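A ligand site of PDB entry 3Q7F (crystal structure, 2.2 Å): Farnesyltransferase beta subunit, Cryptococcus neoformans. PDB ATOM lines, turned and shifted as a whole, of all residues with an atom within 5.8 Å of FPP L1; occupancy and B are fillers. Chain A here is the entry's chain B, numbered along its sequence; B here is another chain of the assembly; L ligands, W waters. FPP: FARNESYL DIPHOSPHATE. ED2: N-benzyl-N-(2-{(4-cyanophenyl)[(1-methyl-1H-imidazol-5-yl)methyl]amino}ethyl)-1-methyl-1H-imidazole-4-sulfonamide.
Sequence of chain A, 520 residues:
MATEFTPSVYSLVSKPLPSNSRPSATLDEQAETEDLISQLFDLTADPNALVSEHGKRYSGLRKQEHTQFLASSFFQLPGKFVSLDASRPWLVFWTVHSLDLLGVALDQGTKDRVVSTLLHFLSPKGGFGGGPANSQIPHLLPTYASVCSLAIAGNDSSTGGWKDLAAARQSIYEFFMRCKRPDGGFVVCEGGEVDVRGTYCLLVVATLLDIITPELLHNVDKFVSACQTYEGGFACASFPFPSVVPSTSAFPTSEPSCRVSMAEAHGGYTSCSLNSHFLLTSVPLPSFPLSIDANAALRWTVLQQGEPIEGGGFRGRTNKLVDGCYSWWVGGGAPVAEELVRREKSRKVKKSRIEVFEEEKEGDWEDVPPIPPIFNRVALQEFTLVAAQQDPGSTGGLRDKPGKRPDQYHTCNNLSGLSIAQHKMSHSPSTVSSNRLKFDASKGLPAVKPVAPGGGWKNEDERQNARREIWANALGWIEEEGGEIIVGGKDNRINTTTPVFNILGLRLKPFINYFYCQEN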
ATOM      1  N   TRP A  90     -20.620  35.124  25.530  1.00  0.00           N
ATOM      2  CA  TRP A  90     -21.032  33.755  25.205  1.00  0.00           C
ATOM      3  C   TRP A  90     -20.019  32.737  25.714  1.00  0.00           C
ATOM      4  O   TRP A  90     -20.402  31.687  26.220  1.00  0.00           O
ATOM      5  CB  TRP A  90     -21.264  33.574  23.706  1.00  0.00           C
ATOM      6  CG  TRP A  90     -22.557  34.147  23.245  1.00  0.00           C
ATOM      7  CD1 TRP A  90     -22.721  35.298  22.528  1.00  0.00           C
ATOM      8  CD2 TRP A  90     -23.858  33.613  23.467  1.00  0.00           C
ATOM      9  NE1 TRP A  90     -24.057  35.507  22.289  1.00  0.00           N
ATOM     10  CE2 TRP A  90     -24.776  34.492  22.856  1.00  0.00           C
ATOM     11  CE3 TRP A  90     -24.349  32.472  24.120  1.00  0.00           C
ATOM     12  CZ2 TRP A  90     -26.165  34.271  22.877  1.00  0.00           C
ATOM     13  CZ3 TRP A  90     -25.729  32.254  24.151  1.00  0.00           C
ATOM     14  CH2 TRP A  90     -26.618  33.153  23.529  1.00  0.00           C
ATOM     15  N   LEU A 141     -27.741  39.845  21.735  1.00  0.00           N
ATOM     16  CA  LEU A 141     -27.248  38.493  22.023  1.00  0.00           C
ATOM     17  C   LEU A 141     -26.286  38.410  23.232  1.00  0.00           C
ATOM     18  O   LEU A 141     -26.531  37.611  24.142  1.00  0.00           O
ATOM     19  CB  LEU A 141     -26.691  37.815  20.758  1.00  0.00           C
ATOM     20  CG  LEU A 141     -27.681  37.090  19.828  1.00  0.00           C
ATOM     21  CD1 LEU A 141     -28.843  37.968  19.344  1.00  0.00           C
ATOM     22  CD2 LEU A 141     -26.946  36.500  18.643  1.00  0.00           C
ATOM     23  N   TYR A 144     -28.288  38.919  26.474  1.00  0.00           N
ATOM     24  CA  TYR A 144     -28.806  37.654  27.007  1.00  0.00           C
ATOM     25  C   TYR A 144     -27.717  36.844  27.701  1.00  0.00           C
ATOM     26  O   TYR A 144     -27.919  36.359  28.819  1.00  0.00           O
ATOM     27  CB  TYR A 144     -29.467  36.808  25.898  1.00  0.00           C
ATOM     28  CG  TYR A 144     -29.652  35.339  26.265  1.00  0.00           C
ATOM     29  CD1 TYR A 144     -30.823  34.902  26.879  1.00  0.00           C
ATOM     30  CD2 TYR A 144     -28.651  34.403  26.004  1.00  0.00           C
ATOM     31  CE1 TYR A 144     -31.005  33.554  27.215  1.00  0.00           C
ATOM     32  CE2 TYR A 144     -28.814  33.049  26.354  1.00  0.00           C
ATOM     33  CZ  TYR A 144     -30.000  32.637  26.964  1.00  0.00           C
ATOM     34  OH  TYR A 144     -30.165  31.312  27.308  1.00  0.00           O
ATOM     35  N   ARG A 197     -33.590  35.476  16.777  1.00  0.00           N
ATOM     36  CA  ARG A 197     -32.629  35.295  17.884  1.00  0.00           C
ATOM     37  C   ARG A 197     -32.599  36.531  18.784  1.00  0.00           C
ATOM     38  O   ARG A 197     -32.473  36.412  20.008  1.00  0.00           O
ATOM     39  CB  ARG A 197     -31.213  35.045  17.371  1.00  0.00           C
ATOM     40  CG  ARG A 197     -30.995  33.731  16.648  1.00  0.00           C
ATOM     41  CD  ARG A 197     -29.575  33.668  16.094  1.00  0.00           C
ATOM     42  NE  ARG A 197     -29.209  34.908  15.411  1.00  0.00           N
ATOM     43  CZ  ARG A 197     -27.974  35.325  15.183  1.00  0.00           C
ATOM     44  NH1 ARG A 197     -26.928  34.607  15.583  1.00  0.00           N
ATOM     45  NH2 ARG A 197     -27.774  36.489  14.568  1.00  0.00           N
ATOM     46  N   TYR A 200     -35.831  36.507  20.859  1.00  0.00           N
ATOM     47  CA  TYR A 200     -35.697  35.556  21.964  1.00  0.00           C
ATOM     48  C   TYR A 200     -34.871  36.146  23.108  1.00  0.00           C
ATOM     49  O   TYR A 200     -35.301  36.132  24.262  1.00  0.00           O
ATOM     50  CB  TYR A 200     -35.097  34.221  21.496  1.00  0.00           C
ATOM     51  CG  TYR A 200     -34.583  33.363  22.644  1.00  0.00           C
ATOM     52  CD1 TYR A 200     -35.478  32.720  23.498  1.00  0.00           C
ATOM     53  CD2 TYR A 200     -33.226  33.238  22.887  1.00  0.00           C
ATOM     54  CE1 TYR A 200     -35.015  31.958  24.574  1.00  0.00           C
ATOM     55  CE2 TYR A 200     -32.751  32.468  23.966  1.00  0.00           C
ATOM     56  CZ  TYR A 200     -33.656  31.839  24.795  1.00  0.00           C
ATOM     57  OH  TYR A 200     -33.208  31.083  25.844  1.00  0.00           O
ATOM     58  N   CYS A 201     -33.691  36.674  22.770  1.00  0.00           N
ATOM     59  CA  CYS A 201     -32.753  37.205  23.755  1.00  0.00           C
ATOM     60  C   CYS A 201     -33.341  38.379  24.525  1.00  0.00           C
ATOM     61  O   CYS A 201     -33.183  38.480  25.742  1.00  0.00           O
ATOM     62  CB  CYS A 201     -31.449  37.594  23.064  1.00  0.00           C
ATOM     63  SG  CYS A 201     -30.457  36.169  22.545  1.00  0.00           S
ATOM     64  N   HIS A 266     -35.294  26.157  10.638  1.00  0.00           N
ATOM     65  CA  HIS A 266     -34.018  25.778  11.214  1.00  0.00           C
ATOM     66  C   HIS A 266     -34.142  25.592  12.724  1.00  0.00           C
ATOM     67  O   HIS A 266     -34.854  26.342  13.387  1.00  0.00           O
ATOM     68  CB  HIS A 266     -32.952  26.840  10.893  1.00  0.00           C
ATOM     69  CG  HIS A 266     -31.557  26.385  11.178  1.00  0.00           C
ATOM     70  ND1 HIS A 266     -30.701  25.940  10.197  1.00  0.00           N
ATOM     71  CD2 HIS A 266     -30.869  26.282  12.346  1.00  0.00           C
ATOM     72  CE1 HIS A 266     -29.552  25.587  10.740  1.00  0.00           C
ATOM     73  NE2 HIS A 266     -29.631  25.784  12.038  1.00  0.00           N
ATOM     74  N   GLY A 267     -33.443  24.589  13.263  1.00  0.00           N
ATOM     75  CA  GLY A 267     -33.463  24.273  14.697  1.00  0.00           C
ATOM     76  C   GLY A 267     -33.197  25.443  15.629  1.00  0.00           C
ATOM     77  O   GLY A 267     -33.895  25.617  16.627  1.00  0.00           O
ATOM     78  N   GLY A 268     -32.192  26.245  15.305  1.00  0.00           N
ATOM     79  CA  GLY A 268     -31.859  27.421  16.094  1.00  0.00           C
ATOM     80  C   GLY A 268     -32.949  28.476  16.129  1.00  0.00           C
ATOM     81  O   GLY A 268     -33.303  28.988  17.200  1.00  0.00           O
ATOM     82  N   TYR A 269     -33.509  28.787  14.969  1.00  0.00           N
ATOM     83  CA  TYR A 269     -34.577  29.775  14.873  1.00  0.00           C
ATOM     84  C   TYR A 269     -35.924  29.235  15.363  1.00  0.00           C
ATOM     85  O   TYR A 269     -36.762  30.003  15.843  1.00  0.00           O
ATOM     86  CB  TYR A 269     -34.678  30.338  13.455  1.00  0.00           C
ATOM     87  CG  TYR A 269     -33.388  30.989  12.988  1.00  0.00           C
ATOM     88  CD1 TYR A 269     -32.859  32.098  13.654  1.00  0.00           C
ATOM     89  CD2 TYR A 269     -32.687  30.485  11.900  1.00  0.00           C
ATOM     90  CE1 TYR A 269     -31.669  32.691  13.240  1.00  0.00           C
ATOM     91  CE2 TYR A 269     -31.501  31.058  11.477  1.00  0.00           C
ATOM     92  CZ  TYR A 269     -30.998  32.159  12.148  1.00  0.00           C
ATOM     93  OH  TYR A 269     -29.823  32.741  11.722  1.00  0.00           O
ATOM     94  N   CYS A 272     -35.695  29.580  19.126  1.00  0.00           N
ATOM     95  CA  CYS A 272     -35.905  30.985  19.475  1.00  0.00           C
ATOM     96  C   CYS A 272     -37.370  31.414  19.322  1.00  0.00           C
ATOM     97  O   CYS A 272     -37.891  32.152  20.161  1.00  0.00           O
ATOM     98  CB  CYS A 272     -34.978  31.893  18.674  1.00  0.00           C
ATOM     99  SG  CYS A 272     -33.241  31.753  19.163  1.00  0.00           S
ATOM    100  N   GLY A 316     -30.437  20.032  12.210  1.00  0.00           N
ATOM    101  CA  GLY A 316     -30.977  21.390  12.318  1.00  0.00           C
ATOM    102  C   GLY A 316     -31.967  21.762  11.232  1.00  0.00           C
ATOM    103  O   GLY A 316     -32.796  22.657  11.429  1.00  0.00           O
ATOM    104  N   ARG A 317     -31.865  21.109  10.092  1.00  0.00           N
ATOM    105  CA  ARG A 317     -32.836  21.264   9.010  1.00  0.00           C
ATOM    106  C   ARG A 317     -32.899  20.014   8.151  1.00  0.00           C
ATOM    107  O   ARG A 317     -31.968  19.209   8.134  1.00  0.00           O
ATOM    108  CB  ARG A 317     -32.564  22.521   8.154  1.00  0.00           C
ATOM    109  CG  ARG A 317     -31.103  22.838   7.931  1.00  0.00           C
ATOM    110  CD  ARG A 317     -30.921  24.150   7.152  1.00  0.00           C
ATOM    111  NE  ARG A 317     -29.513  24.534   7.131  1.00  0.00           N
ATOM    112  CZ  ARG A 317     -28.912  25.189   6.140  1.00  0.00           C
ATOM    113  NH1 ARG A 317     -29.600  25.532   5.058  1.00  0.00           N
ATOM    114  NH2 ARG A 317     -27.622  25.489   6.224  1.00  0.00           N
ATOM    115  N   LYS A 320     -30.059  17.811   6.081  1.00  0.00           N
ATOM    116  CA  LYS A 320     -28.726  18.186   6.541  1.00  0.00           C
ATOM    117  C   LYS A 320     -28.241  17.175   7.590  1.00  0.00           C
ATOM    118  O   LYS A 320     -28.902  16.153   7.818  1.00  0.00           O
ATOM    119  CB  LYS A 320     -28.712  19.627   7.080  1.00  0.00           C
ATOM    120  CG  LYS A 320     -28.917  20.685   6.001  1.00  0.00           C
ATOM    121  CD  LYS A 320     -27.608  20.990   5.285  1.00  0.00           C
ATOM    122  CE  LYS A 320     -27.020  22.293   5.748  1.00  0.00           C
ATOM    123  NZ  LYS A 320     -25.561  22.368   5.535  1.00  0.00           N
ATOM    124  N   LEU A 321     -27.114  17.455   8.230  1.00  0.00           N
ATOM    125  CA  LEU A 321     -26.438  16.468   9.075  1.00  0.00           C
ATOM    126  C   LEU A 321     -26.746  16.653  10.549  1.00  0.00           C
ATOM    127  O   LEU A 321     -26.933  17.788  11.027  1.00  0.00           O
ATOM    128  CB  LEU A 321     -24.923  16.510   8.834  1.00  0.00           C
ATOM    129  CG  LEU A 321     -24.411  16.280   7.404  1.00  0.00           C
ATOM    130  CD1 LEU A 321     -22.907  16.534   7.334  1.00  0.00           C
ATOM    131  CD2 LEU A 321     -24.748  14.875   6.886  1.00  0.00           C
ATOM    132  N   ASP A 323     -26.078  16.978  14.511  1.00  0.00           N
ATOM    133  CA  ASP A 323     -25.113  17.833  15.185  1.00  0.00           C
ATOM    134  C   ASP A 323     -25.501  17.909  16.664  1.00  0.00           C
ATOM    135  O   ASP A 323     -26.655  18.187  16.998  1.00  0.00           O
ATOM    136  CB  ASP A 323     -25.119  19.216  14.540  1.00  0.00           C
ATOM    137  CG  ASP A 323     -24.111  20.172  15.159  1.00  0.00           C
ATOM    138  OD1 ASP A 323     -23.728  20.020  16.341  1.00  0.00           O
ATOM    139  OD2 ASP A 323     -23.717  21.111  14.441  1.00  0.00           O
ATOM    140  N   TYR A 326     -27.761  20.664  18.404  1.00  0.00           N
ATOM    141  CA  TYR A 326     -29.215  20.658  18.196  1.00  0.00           C
ATOM    142  C   TYR A 326     -29.953  19.863  19.268  1.00  0.00           C
ATOM    143  O   TYR A 326     -31.179  19.900  19.349  1.00  0.00           O
ATOM    144  CB  TYR A 326     -29.587  20.198  16.786  1.00  0.00           C
ATOM    145  CG  TYR A 326     -29.055  21.129  15.711  1.00  0.00           C
ATOM    146  CD1 TYR A 326     -29.391  22.477  15.700  1.00  0.00           C
ATOM    147  CD2 TYR A 326     -28.178  20.659  14.721  1.00  0.00           C
ATOM    148  CE1 TYR A 326     -28.892  23.337  14.730  1.00  0.00           C
ATOM    149  CE2 TYR A 326     -27.677  21.508  13.744  1.00  0.00           C
ATOM    150  CZ  TYR A 326     -28.028  22.847  13.758  1.00  0.00           C
ATOM    151  OH  TYR A 326     -27.539  23.699  12.799  1.00  0.00           O
ATOM    152  N   TRP A 329     -31.068  22.998  20.830  1.00  0.00           N
ATOM    153  CA  TRP A 329     -31.933  23.832  19.981  1.00  0.00           C
ATOM    154  C   TRP A 329     -33.230  23.155  19.555  1.00  0.00           C
ATOM    155  O   TRP A 329     -34.299  23.753  19.627  1.00  0.00           O
ATOM    156  CB  TRP A 329     -31.199  24.406  18.763  1.00  0.00           C
ATOM    157  CG  TRP A 329     -29.951  25.166  19.109  1.00  0.00           C
ATOM    158  CD1 TRP A 329     -28.673  24.863  18.726  1.00  0.00           C
ATOM    159  CD2 TRP A 329     -29.853  26.357  19.909  1.00  0.00           C
ATOM    160  NE1 TRP A 329     -27.786  25.788  19.227  1.00  0.00           N
ATOM    161  CE2 TRP A 329     -28.485  26.714  19.948  1.00  0.00           C
ATOM    162  CE3 TRP A 329     -30.789  27.154  20.574  1.00  0.00           C
ATOM    163  CZ2 TRP A 329     -28.024  27.835  20.659  1.00  0.00           C
ATOM    164  CZ3 TRP A 329     -30.329  28.274  21.284  1.00  0.00           C
ATOM    165  CH2 TRP A 329     -28.969  28.604  21.311  1.00  0.00           C
ATOM    166  N   TYR A 409     -18.943  26.085  22.891  1.00  0.00           N
ATOM    167  CA  TYR A 409     -20.312  26.174  22.404  1.00  0.00           C
ATOM    168  C   TYR A 409     -20.983  24.801  22.342  1.00  0.00           C
ATOM    169  O   TYR A 409     -22.124  24.647  22.779  1.00  0.00           O
ATOM    170  CB  TYR A 409     -20.336  26.860  21.025  1.00  0.00           C
ATOM    171  CG  TYR A 409     -21.636  26.702  20.264  1.00  0.00           C
ATOM    172  CD1 TYR A 409     -22.656  27.639  20.399  1.00  0.00           C
ATOM    173  CD2 TYR A 409     -21.835  25.629  19.398  1.00  0.00           C
ATOM    174  CE1 TYR A 409     -23.853  27.503  19.697  1.00  0.00           C
ATOM    175  CE2 TYR A 409     -23.027  25.477  18.697  1.00  0.00           C
ATOM    176  CZ  TYR A 409     -24.029  26.419  18.853  1.00  0.00           C
ATOM    177  OH  TYR A 409     -25.214  26.282  18.170  1.00  0.00           O
ATOM    178  N   TYR B 123     -22.445  36.690   9.443  1.00  0.00           N
ATOM    179  CA  TYR B 123     -23.699  37.457   9.438  1.00  0.00           C
ATOM    180  C   TYR B 123     -23.446  38.878   8.936  1.00  0.00           C
ATOM    181  O   TYR B 123     -24.255  39.438   8.189  1.00  0.00           O
ATOM    182  CB  TYR B 123     -24.265  37.578  10.852  1.00  0.00           C
ATOM    183  CG  TYR B 123     -24.982  36.363  11.403  1.00  0.00           C
ATOM    184  CD1 TYR B 123     -26.356  36.221  11.246  1.00  0.00           C
ATOM    185  CD2 TYR B 123     -24.282  35.375  12.106  1.00  0.00           C
ATOM    186  CE1 TYR B 123     -27.030  35.114  11.756  1.00  0.00           C
ATOM    187  CE2 TYR B 123     -24.945  34.258  12.620  1.00  0.00           C
ATOM    188  CZ  TYR B 123     -26.312  34.130  12.444  1.00  0.00           C
ATOM    189  OH  TYR B 123     -26.984  33.035  12.948  1.00  0.00           O
ATOM    190  N   LYS B 157     -26.285  25.248   0.149  1.00  0.00           N
ATOM    191  CA  LYS B 157     -27.209  25.240   1.286  1.00  0.00           C
ATOM    192  C   LYS B 157     -26.920  26.343   2.304  1.00  0.00           C
ATOM    193  O   LYS B 157     -27.504  26.369   3.393  1.00  0.00           O
ATOM    194  CB  LYS B 157     -27.214  23.867   1.964  1.00  0.00           C
ATOM    195  CG  LYS B 157     -27.628  22.732   1.060  1.00  0.00           C
ATOM    196  CD  LYS B 157     -27.853  21.454   1.825  1.00  0.00           C
ATOM    197  CE  LYS B 157     -28.217  20.315   0.900  1.00  0.00           C
ATOM    198  NZ  LYS B 157     -28.696  19.142   1.675  1.00  0.00           N
ATOM    199  N   ASN B 158     -26.037  27.281   1.945  1.00  0.00           N
ATOM    200  CA  ASN B 158     -25.693  28.399   2.818  1.00  0.00           C
ATOM    201  C   ASN B 158     -26.939  29.161   3.242  1.00  0.00           C
ATOM    202  O   ASN B 158     -27.575  29.831   2.432  1.00  0.00           O
ATOM    203  CB  ASN B 158     -24.692  29.336   2.126  1.00  0.00           C
ATOM    204  CG  ASN B 158     -24.082  30.353   3.084  1.00  0.00           C
ATOM    205  OD1 ASN B 158     -24.788  31.167   3.684  1.00  0.00           O
ATOM    206  ND2 ASN B 158     -22.764  30.313   3.220  1.00  0.00           N
ATOM    207  N   TYR B 159     -27.280  29.042   4.533  1.00  0.00           N
ATOM    208  CA  TYR B 159     -28.520  29.594   5.053  1.00  0.00           C
ATOM    209  C   TYR B 159     -28.624  31.103   4.829  1.00  0.00           C
ATOM    210  O   TYR B 159     -29.639  31.589   4.324  1.00  0.00           O
ATOM    211  CB  TYR B 159     -28.675  29.270   6.546  1.00  0.00           C
ATOM    212  CG  TYR B 159     -30.083  29.499   7.068  1.00  0.00           C
ATOM    213  CD1 TYR B 159     -31.017  28.468   7.091  1.00  0.00           C
ATOM    214  CD2 TYR B 159     -30.486  30.761   7.516  1.00  0.00           C
ATOM    215  CE1 TYR B 159     -32.305  28.664   7.562  1.00  0.00           C
ATOM    216  CE2 TYR B 159     -31.774  30.981   7.989  1.00  0.00           C
ATOM    217  CZ  TYR B 159     -32.678  29.928   8.013  1.00  0.00           C
ATOM    218  OH  TYR B 159     -33.964  30.137   8.479  1.00  0.00           O
ATOM    219  N   HIS B 160     -27.562  31.831   5.179  1.00  0.00           N
ATOM    220  CA  HIS B 160     -27.541  33.286   5.047  1.00  0.00           C
ATOM    221  C   HIS B 160     -27.702  33.758   3.611  1.00  0.00           C
ATOM    222  O   HIS B 160     -28.345  34.776   3.362  1.00  0.00           O
ATOM    223  CB  HIS B 160     -26.267  33.887   5.656  1.00  0.00           C
ATOM    224  CG  HIS B 160     -26.143  33.672   7.129  1.00  0.00           C
ATOM    225  ND1 HIS B 160     -27.238  33.486   7.953  1.00  0.00           N
ATOM    226  CD2 HIS B 160     -25.058  33.628   7.942  1.00  0.00           C
ATOM    227  CE1 HIS B 160     -26.833  33.326   9.195  1.00  0.00           C
ATOM    228  NE2 HIS B 160     -25.515  33.407   9.219  1.00  0.00           N
HETATM  229  C1  FPP L   1     -26.510  27.235  10.166  1.00  0.00           C
HETATM  230  O1  FPP L   1     -25.224  26.928   9.778  1.00  0.00           O
HETATM  231  C2  FPP L   1     -26.492  28.520  10.929  1.00  0.00           C
HETATM  232  C3  FPP L   1     -27.644  29.146  11.325  1.00  0.00           C
HETATM  233  C4  FPP L   1     -28.466  29.825  10.289  1.00  0.00           C
HETATM  234  C5  FPP L   1     -27.717  29.694  12.710  1.00  0.00           C
HETATM  235  C6  FPP L   1     -28.545  28.806  13.582  1.00  0.00           C
HETATM  236  C7  FPP L   1     -29.107  29.615  14.717  1.00  0.00           C
HETATM  237  C8  FPP L   1     -28.901  29.296  16.041  1.00  0.00           C
HETATM  238  C10 FPP L   1     -28.375  27.954  16.430  1.00  0.00           C
HETATM  239  C9  FPP L   1     -29.697  30.069  17.050  1.00  0.00           C
HETATM  240  C11 FPP L   1     -28.853  30.520  18.194  1.00  0.00           C
HETATM  241  C12 FPP L   1     -29.677  31.352  19.114  1.00  0.00           C
HETATM  242  C13 FPP L   1     -29.122  32.273  19.967  1.00  0.00           C
HETATM  243  C14 FPP L   1     -29.889  32.703  21.170  1.00  0.00           C
HETATM  244  C15 FPP L   1     -27.825  32.928  19.644  1.00  0.00           C
HETATM  245  PA  FPP L   1     -24.829  25.531   9.208  1.00  0.00           P
HETATM  246  O1A FPP L   1     -25.255  25.461   7.724  1.00  0.00           O
HETATM  247  O2A FPP L   1     -23.292  25.398   9.295  1.00  0.00           O
HETATM  248  O3A FPP L   1     -25.485  24.418  10.083  1.00  0.00           O
HETATM  249  PB  FPP L   1     -26.451  23.305   9.554  1.00  0.00           P
HETATM  250  O1B FPP L   1     -25.796  22.543   8.422  1.00  0.00           O
HETATM  251  O2B FPP L   1     -26.716  22.355  10.688  1.00  0.00           O
HETATM  252  O3B FPP L   1     -27.740  23.920   9.066  1.00  0.00           O
HETATM  253  CAB ED2 L   2     -19.855  24.716  12.476  1.00  0.00           C
HETATM  254  NBH ED2 L   2     -20.822  24.826  13.574  1.00  0.00           N
HETATM  255  CAQ ED2 L   2     -21.569  23.786  14.078  1.00  0.00           C
HETATM  256  NAX ED2 L   2     -22.373  24.262  14.996  1.00  0.00           N
HETATM  257  CAP ED2 L   2     -21.932  25.549  15.312  1.00  0.00           C
HETATM  258  CBC ED2 L   2     -21.018  25.921  14.383  1.00  0.00           C
HETATM  259  CAW ED2 L   2     -20.326  27.238  14.285  1.00  0.00           C
HETATM  260  NBE ED2 L   2     -20.534  28.096  15.460  1.00  0.00           N
HETATM  261  CBB ED2 L   2     -19.661  28.058  16.559  1.00  0.00           C
HETATM  262  CAN ED2 L   2     -19.657  29.100  17.493  1.00  0.00           C
HETATM  263  CAL ED2 L   2     -18.772  29.047  18.700  1.00  0.00           C
HETATM  264  CAZ ED2 L   2     -17.937  28.004  18.864  1.00  0.00           C
HETATM  265  CAF ED2 L   2     -17.034  27.939  20.070  1.00  0.00           C
HETATM  266  NAC ED2 L   2     -16.341  27.879  20.996  1.00  0.00           N
HETATM  267  CAM ED2 L   2     -17.922  26.904  17.867  1.00  0.00           C
HETATM  268  CAO ED2 L   2     -18.780  26.951  16.743  1.00  0.00           C
HETATM  269  CAT ED2 L   2     -21.524  29.219  15.315  1.00  0.00           C
HETATM  270  CAU ED2 L   2     -22.586  29.119  16.415  1.00  0.00           C
HETATM  271  NBF ED2 L   2     -23.502  30.297  16.418  1.00  0.00           N
HETATM  272  SBI ED2 L   2     -24.879  30.055  15.530  1.00  0.00           S
HETATM  273  OAD ED2 L   2     -25.974  30.177  16.467  1.00  0.00           O
HETATM  274  OAE ED2 L   2     -25.029  31.059  14.498  1.00  0.00           O
HETATM  275  CBD ED2 L   2     -24.917  28.425  14.870  1.00  0.00           C
HETATM  276  CAS ED2 L   2     -24.295  27.975  13.661  1.00  0.00           C
HETATM  277  NBG ED2 L   2     -24.541  26.579  13.585  1.00  0.00           N
HETATM  278  CAA ED2 L   2     -24.093  25.686  12.542  1.00  0.00           C
HETATM  279  CAR ED2 L   2     -25.292  26.206  14.718  1.00  0.00           C
HETATM  280  NAY ED2 L   2     -25.482  27.325  15.478  1.00  0.00           N
HETATM  281  CAV ED2 L   2     -22.861  31.594  16.122  1.00  0.00           C
HETATM  282  CBA ED2 L   2     -22.624  32.310  17.425  1.00  0.00           C
HETATM  283  CAJ ED2 L   2     -23.636  32.410  18.366  1.00  0.00           C
HETATM  284  CAH ED2 L   2     -23.405  33.063  19.551  1.00  0.00           C
HETATM  285  CAG ED2 L   2     -22.144  33.611  19.809  1.00  0.00           C
HETATM  286  CAI ED2 L   2     -21.136  33.493  18.896  1.00  0.00           C
HETATM  287  CAK ED2 L   2     -21.368  32.850  17.681  1.00  0.00           C
HETATM  288  O   HOH W   1     -28.274  20.130  10.479  1.00  0.00           O
HETATM  289  O   HOH W   2     -24.287  21.682  11.983  1.00  0.00           O
HETATM  290  O   HOH W   3     -25.375  19.906   8.473  1.00  0.00           O
HETATM  291  O   HOH W   4     -25.492  27.708   6.251  1.00  0.00           O
HETATM  292  O   HOH W   5     -24.649  25.124   4.341  1.00  0.00           O
HETATM  293  O   HOH W   6     -22.482  23.227  10.740  1.00  0.00           O
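Trp 90 touches FPP L1. Leu 141 touches FPP L1 (CD2 to C15, 3.8 Å). Arg 197 touches FPP L1. Tyr 200 touches FPP L1. Cys 201 touches FPP L1 (SG to C14, 3.8 Å). His 266 touches FPP L1. Gly 268 touches FPP L1 (CA to C8, 3.5 Å). Tyr 269 touches FPP L1. Cys 272 touches FPP L1 (SG to C12, 3.6 Å). NE1 of Trp 329 touches C10 of FPP L1 (3.6 Å). OH of Tyr 409 touches C10 of FPP L1, 3.98 Å away. Tyr 123 of chain B touches FPP L1 (OH to C5, 3.4 Å). CD2 of Tyr 159 of chain B touches C4 of FPP L1, at 3.6 Å. Hydrophobic or aromatic side chains that line FPP L1: Trp 90, Leu 141, Tyr 200, His 266, Tyr 269, Tyr 326, Trp 329 and Tyr 159 of chain B. Of the 24 residues printed, 16 come within 4 Å of FPP L1. The nearest printed residue that does not touch FPP L1 is His 160 of chain B (4.02 Å).
The side-chain hydroxyl of Tyr 326 lies within hydrogen-bond range of an oxygen (O2B) of FPP L1. O3B of FPP L1 lies within salt-bridge range of NE of Arg 317 (2.7 Å). The side-chain amino group (NZ) of Lys 320 is in salt-bridge range of an oxygen (O1B) of FPP L1 (2.9 Å). An oxygen (OAE) of ED2 L2 is in hydrogen-bond range of the side-chain hydroxyl (OH) of Tyr 123 of chain B, at 3.2 Å. NAY of ED2 L2 lies within hydrogen-bond range of OH of Tyr 409 (2.9 Å).
OH of Tyr 326 sits at hydrogen-bond distance from NE2 of His 266 (3.1 Å). The guanidinium group (NH1) of Arg 317 is in hydrogen-bond range of the backbone carbonyl oxygen (O) of Lys 157 of chain B, at 2.8 Å. The side-chain hydroxyl of Tyr 269 sits at hydrogen-bond distance from the side-chain hydroxyl of Tyr 123 of chain B (3.1 Å). The guanidinium group (NH1) of Arg 197 sits at hydrogen-bond distance from the side-chain hydroxyl (OH) of Tyr 123 of chain B (3.1 Å). The backbone carbonyl oxygen of Gly 268 lies within hydrogen-bond range of the side-chain sulfur of Cys 272 (3.4 Å). The side-chain hydroxyl of Tyr 409 sits at hydrogen-bond distance from the indole nitrogen of Trp 329 (2.8 Å). The backbone carbonyl oxygen (O) of Arg 197 sits at hydrogen-bond distance from the side-chain sulfur (SG) of Cys 201. OH of Tyr 200 lies within hydrogen-bond range of OH of Tyr 144 (3.4 Å).
Water W3 bridges O1B of FPP L1 (2.7 Å) and N of Leu 321 (3.0 Å). Water W4 lies within hydrogen-bond range of an oxygen (O1A) of FPP L1, the backbone NH of Tyr 159 of chain B and the guanidinium group of Arg 317. Water W1 lies within hydrogen-bond range of an oxygen (O2B) of FPP L1 (2.7 Å), the backbone carbonyl oxygen of Leu 321 (2.8 Å) and the backbone NH of Gly 316 (2.8 Å). Water W5 lies within hydrogen-bond range of NZ of Lys 320 (3.1 Å), O of Lys 157 of chain B (3.3 Å) and O1A of FPP L1 (3.5 Å).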
